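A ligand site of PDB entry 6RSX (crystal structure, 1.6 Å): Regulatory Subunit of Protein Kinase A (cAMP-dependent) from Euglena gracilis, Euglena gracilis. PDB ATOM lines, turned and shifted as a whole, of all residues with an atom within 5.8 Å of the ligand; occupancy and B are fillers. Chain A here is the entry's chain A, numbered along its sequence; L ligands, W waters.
The side-chain carboxylate (OE2) of Glu 115 sits at hydrogen-bond distance from the side-chain hydroxyl (OH) of Tyr 175, 2.7 Å away. The backbone carbonyl oxygen of Gly 114 is in hydrogen-bond range of the guanidinium group of Arg 124 (2.9 Å). NE of Arg 124 lies within hydrogen-bond range of SD of Met 72 (3.6 Å). O of Met 72 sits at hydrogen-bond distance from N of Val 128, 3.0 Å away. The backbone carbonyl oxygen of Ser 105 is in hydrogen-bond range of the backbone NH of Ile 91, at 2.8 Å. The backbone NH (N) of Lys 104 is in hydrogen-bond range of the backbone carbonyl oxygen (O) of Ile 91 (2.8 Å).
OE1 of Glu 115 lies within hydrogen-bond range of O6 of the ligand (2.6 Å). NH1 of Arg 124 is in salt-bridge range of O1 of the ligand, at 2.8 Å. An oxygen (O2) of the ligand lies within hydrogen-bond range of the backbone NH of Ala 125. The backbone NH of Ala 117 is in hydrogen-bond range of an oxygen (O1) of the ligand. The backbone NH (N) of Gly 114 lies within hydrogen-bond range of an oxygen (O6) of the ligand (2.9 Å). The side-chain hydroxyl (OH) of Tyr 175 is in hydrogen-bond range of an oxygen (O6) of the ligand (3.2 Å). N of Leu 116 lies within hydrogen-bond range of O1 of the ligand, at 3.4 Å.
Water W6 lies within hydrogen-bond range of the side-chain hydroxyl of Thr 122 (2.7 Å), the backbone carbonyl oxygen of Pro 123 (2.7 Å) and an oxygen (O2) of the ligand (2.9 Å). Water W2 bridges OG of Ser 105 (2.6 Å) and N2 of the ligand (2.9 Å). Water W1 lies within hydrogen-bond range of O of Ser 112, OH of Tyr 175 and O6 of the ligand. Water W5 bridges the side-chain hydroxyl of Thr 173 (2.8 Å) and a nitrogen (N3) of the ligand (3.4 Å).
An oxygen (O3) of the ligand sits close to the side-chain sulfur (SD) of Met 72 (3.4 Å). Ile 91 touches the ligand (CG2 to N2, 3.6 Å). CD1 of Ile 93 touches N4 of the ligand (3.7 Å). Phe 113 touches the ligand. Ala 126 touches the ligand (O to C1, 3.5 Å). Hydrophobic or aromatic side chains that line the ligand: Met 72, Ile 91, Ile 93, Phe 113, Leu 116, Ala 117, Ala 125, Ala 126 and Tyr 175.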
ATOM      1  N   MET A  72      19.910  30.381 -26.190  1.00  0.00           N
ATOM      2  CA  MET A  72      19.232  29.962 -24.966  1.00  0.00           C
ATOM      3  C   MET A  72      20.125  30.304 -23.784  1.00  0.00           C
ATOM      4  O   MET A  72      21.345  30.398 -23.914  1.00  0.00           O
ATOM      5  CB  MET A  72      18.902  28.480 -24.958  1.00  0.00           C
ATOM      6  CG  MET A  72      20.170  27.550 -25.054  1.00  0.00           C
ATOM      7  SD  MET A  72      19.699  25.794 -25.029  1.00  0.00           S
ATOM      8  CE  MET A  72      18.791  25.684 -26.557  1.00  0.00           C
ATOM      9  N   ILE A  91      29.343  27.054 -25.576  1.00  0.00           N
ATOM     10  CA  ILE A  91      28.599  26.448 -24.480  1.00  0.00           C
ATOM     11  C   ILE A  91      29.183  27.014 -23.192  1.00  0.00           C
ATOM     12  O   ILE A  91      30.386  26.861 -22.913  1.00  0.00           O
ATOM     13  CB  ILE A  91      28.737  24.917 -24.499  1.00  0.00           C
ATOM     14  CG1 ILE A  91      28.306  24.329 -25.834  1.00  0.00           C
ATOM     15  CG2 ILE A  91      27.982  24.310 -23.304  1.00  0.00           C
ATOM     16  CD1 ILE A  91      26.863  24.729 -26.300  1.00  0.00           C
ATOM     17  N   ILE A  93      28.586  27.458 -18.912  1.00  0.00           N
ATOM     18  CA  ILE A  93      27.880  26.879 -17.776  1.00  0.00           C
ATOM     19  C   ILE A  93      28.261  27.608 -16.495  1.00  0.00           C
ATOM     20  O   ILE A  93      29.440  27.725 -16.162  1.00  0.00           O
ATOM     21  CB  ILE A  93      28.127  25.365 -17.645  1.00  0.00           C
ATOM     22  CG1 ILE A  93      27.684  24.650 -18.936  1.00  0.00           C
ATOM     23  CG2 ILE A  93      27.380  24.804 -16.376  1.00  0.00           C
ATOM     24  CD1 ILE A  93      28.036  23.137 -18.958  1.00  0.00           C
ATOM     25  N   LYS A 104      32.848  26.211 -21.677  1.00  0.00           N
ATOM     26  CA  LYS A 104      33.027  24.759 -21.644  1.00  0.00           C
ATOM     27  C   LYS A 104      33.486  24.181 -22.980  1.00  0.00           C
ATOM     28  O   LYS A 104      34.403  23.341 -23.000  1.00  0.00           O
ATOM     29  CB  LYS A 104      31.735  24.048 -21.203  1.00  0.00           C
ATOM     30  CG  LYS A 104      31.325  24.299 -19.739  1.00  0.00           C
ATOM     31  CD  LYS A 104      32.356  23.762 -18.766  1.00  0.00           C
ATOM     32  CE  LYS A 104      32.145  24.240 -17.334  1.00  0.00           C
ATOM     33  NZ  LYS A 104      33.074  23.505 -16.402  1.00  0.00           N
ATOM     34  N   SER A 105      32.904  24.620 -24.098  1.00  0.00           N
ATOM     35  CA  SER A 105      33.279  24.106 -25.409  1.00  0.00           C
ATOM     36  C   SER A 105      32.713  25.033 -26.460  1.00  0.00           C
ATOM     37  O   SER A 105      31.857  25.893 -26.175  1.00  0.00           O
ATOM     38  CB  SER A 105      32.785  22.668 -25.627  1.00  0.00           C
ATOM     39  OG  SER A 105      31.365  22.613 -25.733  1.00  0.00           O
ATOM     40  N   SER A 112      24.395  19.428 -32.531  1.00  0.00           N
ATOM     41  CA  SER A 112      23.060  19.750 -32.012  1.00  0.00           C
ATOM     42  C   SER A 112      23.183  20.147 -30.552  1.00  0.00           C
ATOM     43  O   SER A 112      24.163  19.806 -29.860  1.00  0.00           O
ATOM     44  CB  SER A 112      22.137  18.556 -32.212  1.00  0.00           C
ATOM     45  OG  SER A 112      22.695  17.380 -31.640  1.00  0.00           O
ATOM     46  N   PHE A 113      22.146  20.834 -30.071  1.00  0.00           N
ATOM     47  CA  PHE A 113      22.042  21.219 -28.669  1.00  0.00           C
ATOM     48  C   PHE A 113      20.578  21.456 -28.305  1.00  0.00           C
ATOM     49  O   PHE A 113      19.745  21.872 -29.144  1.00  0.00           O
ATOM     50  CB  PHE A 113      22.887  22.470 -28.315  1.00  0.00           C
ATOM     51  CG  PHE A 113      22.555  23.673 -29.096  1.00  0.00           C
ATOM     52  CD1 PHE A 113      23.138  23.910 -30.346  1.00  0.00           C
ATOM     53  CD2 PHE A 113      21.685  24.651 -28.584  1.00  0.00           C
ATOM     54  CE1 PHE A 113      22.826  25.062 -31.075  1.00  0.00           C
ATOM     55  CE2 PHE A 113      21.384  25.794 -29.296  1.00  0.00           C
ATOM     56  CZ  PHE A 113      21.947  26.010 -30.563  1.00  0.00           C
ATOM     57  N   GLY A 114      20.294  21.252 -27.028  1.00  0.00           N
ATOM     58  CA  GLY A 114      18.991  21.581 -26.466  1.00  0.00           C
ATOM     59  C   GLY A 114      18.110  20.375 -26.217  1.00  0.00           C
ATOM     60  O   GLY A 114      16.920  20.536 -25.958  1.00  0.00           O
ATOM     61  N   GLU A 115      18.669  19.176 -26.245  1.00  0.00           N
ATOM     62  CA  GLU A 115      17.845  17.988 -26.092  1.00  0.00           C
ATOM     63  C   GLU A 115      17.508  17.702 -24.616  1.00  0.00           C
ATOM     64  O   GLU A 115      16.459  17.104 -24.360  1.00  0.00           O
ATOM     65  CB  GLU A 115      18.564  16.771 -26.724  1.00  0.00           C
ATOM     66  CG  GLU A 115      19.592  16.079 -25.872  1.00  0.00           C
ATOM     67  CD  GLU A 115      20.978  16.742 -25.872  1.00  0.00           C
ATOM     68  OE1 GLU A 115      21.151  17.812 -26.501  1.00  0.00           O
ATOM     69  OE2 GLU A 115      21.864  16.182 -25.200  1.00  0.00           O
ATOM     70  N   LEU A 116      18.373  18.092 -23.673  1.00  0.00           N
ATOM     71  CA  LEU A 116      18.205  17.636 -22.288  1.00  0.00           C
ATOM     72  C   LEU A 116      16.895  18.162 -21.706  1.00  0.00           C
ATOM     73  O   LEU A 116      16.130  17.397 -21.103  1.00  0.00           O
ATOM     74  CB  LEU A 116      19.348  18.109 -21.426  1.00  0.00           C
ATOM     75  CG  LEU A 116      20.762  17.523 -21.749  1.00  0.00           C
ATOM     76  CD1 LEU A 116      21.775  18.123 -20.808  1.00  0.00           C
ATOM     77  CD2 LEU A 116      20.746  16.003 -21.660  1.00  0.00           C
ATOM     78  N   ALA A 117      16.627  19.453 -21.909  1.00  0.00           N
ATOM     79  CA  ALA A 117      15.378  20.037 -21.352  1.00  0.00           C
ATOM     80  C   ALA A 117      14.147  19.362 -21.942  1.00  0.00           C
ATOM     81  O   ALA A 117      13.128  19.169 -21.251  1.00  0.00           O
ATOM     82  CB  ALA A 117      15.342  21.547 -21.627  1.00  0.00           C
ATOM     83  N   LEU A 118      14.194  19.034 -23.237  1.00  0.00           N
ATOM     84  CA  LEU A 118      13.066  18.406 -23.894  1.00  0.00           C
ATOM     85  C   LEU A 118      12.912  16.941 -23.481  1.00  0.00           C
ATOM     86  O   LEU A 118      11.796  16.430 -23.443  1.00  0.00           O
ATOM     87  CB  LEU A 118      13.153  18.532 -25.402  1.00  0.00           C
ATOM     88  CG  LEU A 118      13.410  19.924 -26.032  1.00  0.00           C
ATOM     89  CD1 LEU A 118      13.093  20.094 -27.556  1.00  0.00           C
ATOM     90  CD2 LEU A 118      12.959  21.086 -25.265  1.00  0.00           C
ATOM     91  N   THR A 122      13.991  19.210 -17.451  1.00  0.00           N
ATOM     92  CA  THR A 122      14.876  20.022 -16.624  1.00  0.00           C
ATOM     93  C   THR A 122      15.039  21.409 -17.246  1.00  0.00           C
ATOM     94  O   THR A 122      14.869  21.565 -18.463  1.00  0.00           O
ATOM     95  CB  THR A 122      16.252  19.361 -16.494  1.00  0.00           C
ATOM     96  OG1 THR A 122      16.703  18.980 -17.810  1.00  0.00           O
ATOM     97  CG2 THR A 122      16.195  18.114 -15.604  1.00  0.00           C
ATOM     98  N   PRO A 123      15.339  22.441 -16.460  1.00  0.00           N
ATOM     99  CA  PRO A 123      15.734  23.724 -17.052  1.00  0.00           C
ATOM    100  C   PRO A 123      17.006  23.530 -17.870  1.00  0.00           C
ATOM    101  O   PRO A 123      17.785  22.617 -17.612  1.00  0.00           O
ATOM    102  CB  PRO A 123      16.043  24.593 -15.835  1.00  0.00           C
ATOM    103  CG  PRO A 123      15.305  23.893 -14.648  1.00  0.00           C
ATOM    104  CD  PRO A 123      15.494  22.428 -14.994  1.00  0.00           C
ATOM    105  N   ARG A 124      17.222  24.436 -18.836  1.00  0.00           N
ATOM    106  CA  ARG A 124      18.478  24.331 -19.636  1.00  0.00           C
ATOM    107  C   ARG A 124      19.711  24.202 -18.759  1.00  0.00           C
ATOM    108  O   ARG A 124      19.918  24.969 -17.793  1.00  0.00           O
ATOM    109  CB  ARG A 124      18.650  25.573 -20.530  1.00  0.00           C
ATOM    110  CG  ARG A 124      17.570  25.865 -21.582  1.00  0.00           C
ATOM    111  CD  ARG A 124      17.322  24.693 -22.543  1.00  0.00           C
ATOM    112  NE  ARG A 124      16.454  25.110 -23.641  1.00  0.00           N
ATOM    113  CZ  ARG A 124      16.158  24.328 -24.659  1.00  0.00           C
ATOM    114  NH1 ARG A 124      16.674  23.089 -24.689  1.00  0.00           N
ATOM    115  NH2 ARG A 124      15.391  24.805 -25.653  1.00  0.00           N
ATOM    116  N   ALA A 125      20.631  23.299 -19.135  1.00  0.00           N
ATOM    117  CA  ALA A 125      21.862  23.058 -18.371  1.00  0.00           C
ATOM    118  C   ALA A 125      23.036  23.985 -18.739  1.00  0.00           C
ATOM    119  O   ALA A 125      24.062  23.993 -18.055  1.00  0.00           O
ATOM    120  CB  ALA A 125      22.308  21.582 -18.540  1.00  0.00           C
ATOM    121  N   ALA A 126      22.903  24.770 -19.809  1.00  0.00           N
ATOM    122  CA  ALA A 126      23.975  25.619 -20.265  1.00  0.00           C
ATOM    123  C   ALA A 126      23.355  26.762 -21.042  1.00  0.00           C
ATOM    124  O   ALA A 126      22.248  26.616 -21.592  1.00  0.00           O
ATOM    125  CB  ALA A 126      24.946  24.811 -21.152  1.00  0.00           C
ATOM    126  N   SER A 127      24.082  27.871 -21.110  1.00  0.00           N
ATOM    127  CA  SER A 127      23.786  28.892 -22.094  1.00  0.00           C
ATOM    128  C   SER A 127      24.489  28.549 -23.409  1.00  0.00           C
ATOM    129  O   SER A 127      25.596  27.976 -23.410  1.00  0.00           O
ATOM    130  CB  SER A 127      24.256  30.252 -21.600  1.00  0.00           C
ATOM    131  OG  SER A 127      23.578  30.645 -20.375  1.00  0.00           O
ATOM    132  N   VAL A 128      23.903  28.966 -24.524  1.00  0.00           N
ATOM    133  CA  VAL A 128      24.527  28.762 -25.837  1.00  0.00           C
ATOM    134  C   VAL A 128      24.557  30.113 -26.538  1.00  0.00           C
ATOM    135  O   VAL A 128      23.489  30.680 -26.839  1.00  0.00           O
ATOM    136  CB  VAL A 128      23.770  27.732 -26.684  1.00  0.00           C
ATOM    137  CG1 VAL A 128      24.499  27.472 -28.032  1.00  0.00           C
ATOM    138  CG2 VAL A 128      23.591  26.438 -25.911  1.00  0.00           C
ATOM    139  N   THR A 173      33.524  13.725 -19.136  1.00  0.00           N
ATOM    140  CA  THR A 173      32.528  14.338 -18.275  1.00  0.00           C
ATOM    141  C   THR A 173      31.186  13.617 -18.393  1.00  0.00           C
ATOM    142  O   THR A 173      30.950  12.820 -19.313  1.00  0.00           O
ATOM    143  CB  THR A 173      32.311  15.804 -18.649  1.00  0.00           C
ATOM    144  OG1 THR A 173      31.781  15.845 -19.977  1.00  0.00           O
ATOM    145  CG2 THR A 173      33.609  16.551 -18.615  1.00  0.00           C
ATOM    146  N   TYR A 175      28.371  14.797 -19.407  1.00  0.00           N
ATOM    147  CA  TYR A 175      27.694  15.036 -20.677  1.00  0.00           C
ATOM    148  C   TYR A 175      28.428  14.346 -21.828  1.00  0.00           C
ATOM    149  O   TYR A 175      27.790  13.855 -22.772  1.00  0.00           O
ATOM    150  CB  TYR A 175      27.573  16.531 -20.982  1.00  0.00           C
ATOM    151  CG  TYR A 175      26.710  16.758 -22.173  1.00  0.00           C
ATOM    152  CD1 TYR A 175      25.327  16.544 -22.111  1.00  0.00           C
ATOM    153  CD2 TYR A 175      27.233  17.237 -23.356  1.00  0.00           C
ATOM    154  CE1 TYR A 175      24.521  16.718 -23.221  1.00  0.00           C
ATOM    155  CE2 TYR A 175      26.454  17.408 -24.481  1.00  0.00           C
ATOM    156  CZ  TYR A 175      25.085  17.197 -24.408  1.00  0.00           C
ATOM    157  OH  TYR A 175      24.296  17.375 -25.540  1.00  0.00           O
HETATM  158  P1  LIG L   1      19.744  21.639 -22.614  1.00  0.00           P
HETATM  159  O1  LIG L   1      18.274  21.473 -23.112  1.00  0.00           O
HETATM  160  O2  LIG L   1      20.155  21.481 -21.204  1.00  0.00           O
HETATM  161  O3  LIG L   1      20.241  23.124 -22.977  1.00  0.00           O
HETATM  162  C1  LIG L   1      21.627  23.442 -23.049  1.00  0.00           C
HETATM  163  C2  LIG L   1      22.264  22.413 -23.943  1.00  0.00           C
HETATM  164  O4  LIG L   1      23.683  22.521 -24.055  1.00  0.00           O
HETATM  165  C3  LIG L   1      22.076  21.000 -23.461  1.00  0.00           C
HETATM  166  O5  LIG L   1      20.729  20.592 -23.540  1.00  0.00           O
HETATM  167  C4  LIG L   1      23.056  20.218 -24.337  1.00  0.00           C
HETATM  168  O6  LIG L   1      22.417  19.921 -25.570  1.00  0.00           O
HETATM  169  C5  LIG L   1      24.164  21.274 -24.577  1.00  0.00           C
HETATM  170  N1  LIG L   1      25.425  20.984 -23.914  1.00  0.00           N
HETATM  171  C6  LIG L   1      26.665  21.021 -24.520  1.00  0.00           C
HETATM  172  N2  LIG L   1      27.586  20.762 -23.611  1.00  0.00           N
HETATM  173  C7  LIG L   1      26.940  20.531 -22.462  1.00  0.00           C
HETATM  174  C8  LIG L   1      27.462  20.185 -21.244  1.00  0.00           C
HETATM  175  N3  LIG L   1      28.820  19.977 -20.818  1.00  0.00           N
HETATM  176  N4  LIG L   1      26.686  19.954 -20.212  1.00  0.00           N
HETATM  177  C9  LIG L   1      25.340  20.111 -20.376  1.00  0.00           C
HETATM  178  N5  LIG L   1      24.784  20.442 -21.587  1.00  0.00           N
HETATM  179  C10 LIG L   1      25.608  20.661 -22.629  1.00  0.00           C
HETATM  180  O   HOH W   1      25.258  19.597 -27.372  1.00  0.00           O
HETATM  181  O   HOH W   2      30.436  21.334 -23.661  1.00  0.00           O
HETATM  182  O   HOH W   3      30.408  19.254 -18.604  1.00  0.00           O
HETATM  183  O   HOH W   4      26.902  18.970 -17.683  1.00  0.00           O
HETATM  184  O   HOH W   5      31.847  18.416 -21.052  1.00  0.00           O
HETATM  185  O   HOH W   6      18.536  20.461 -19.069  1.00  0.00           O
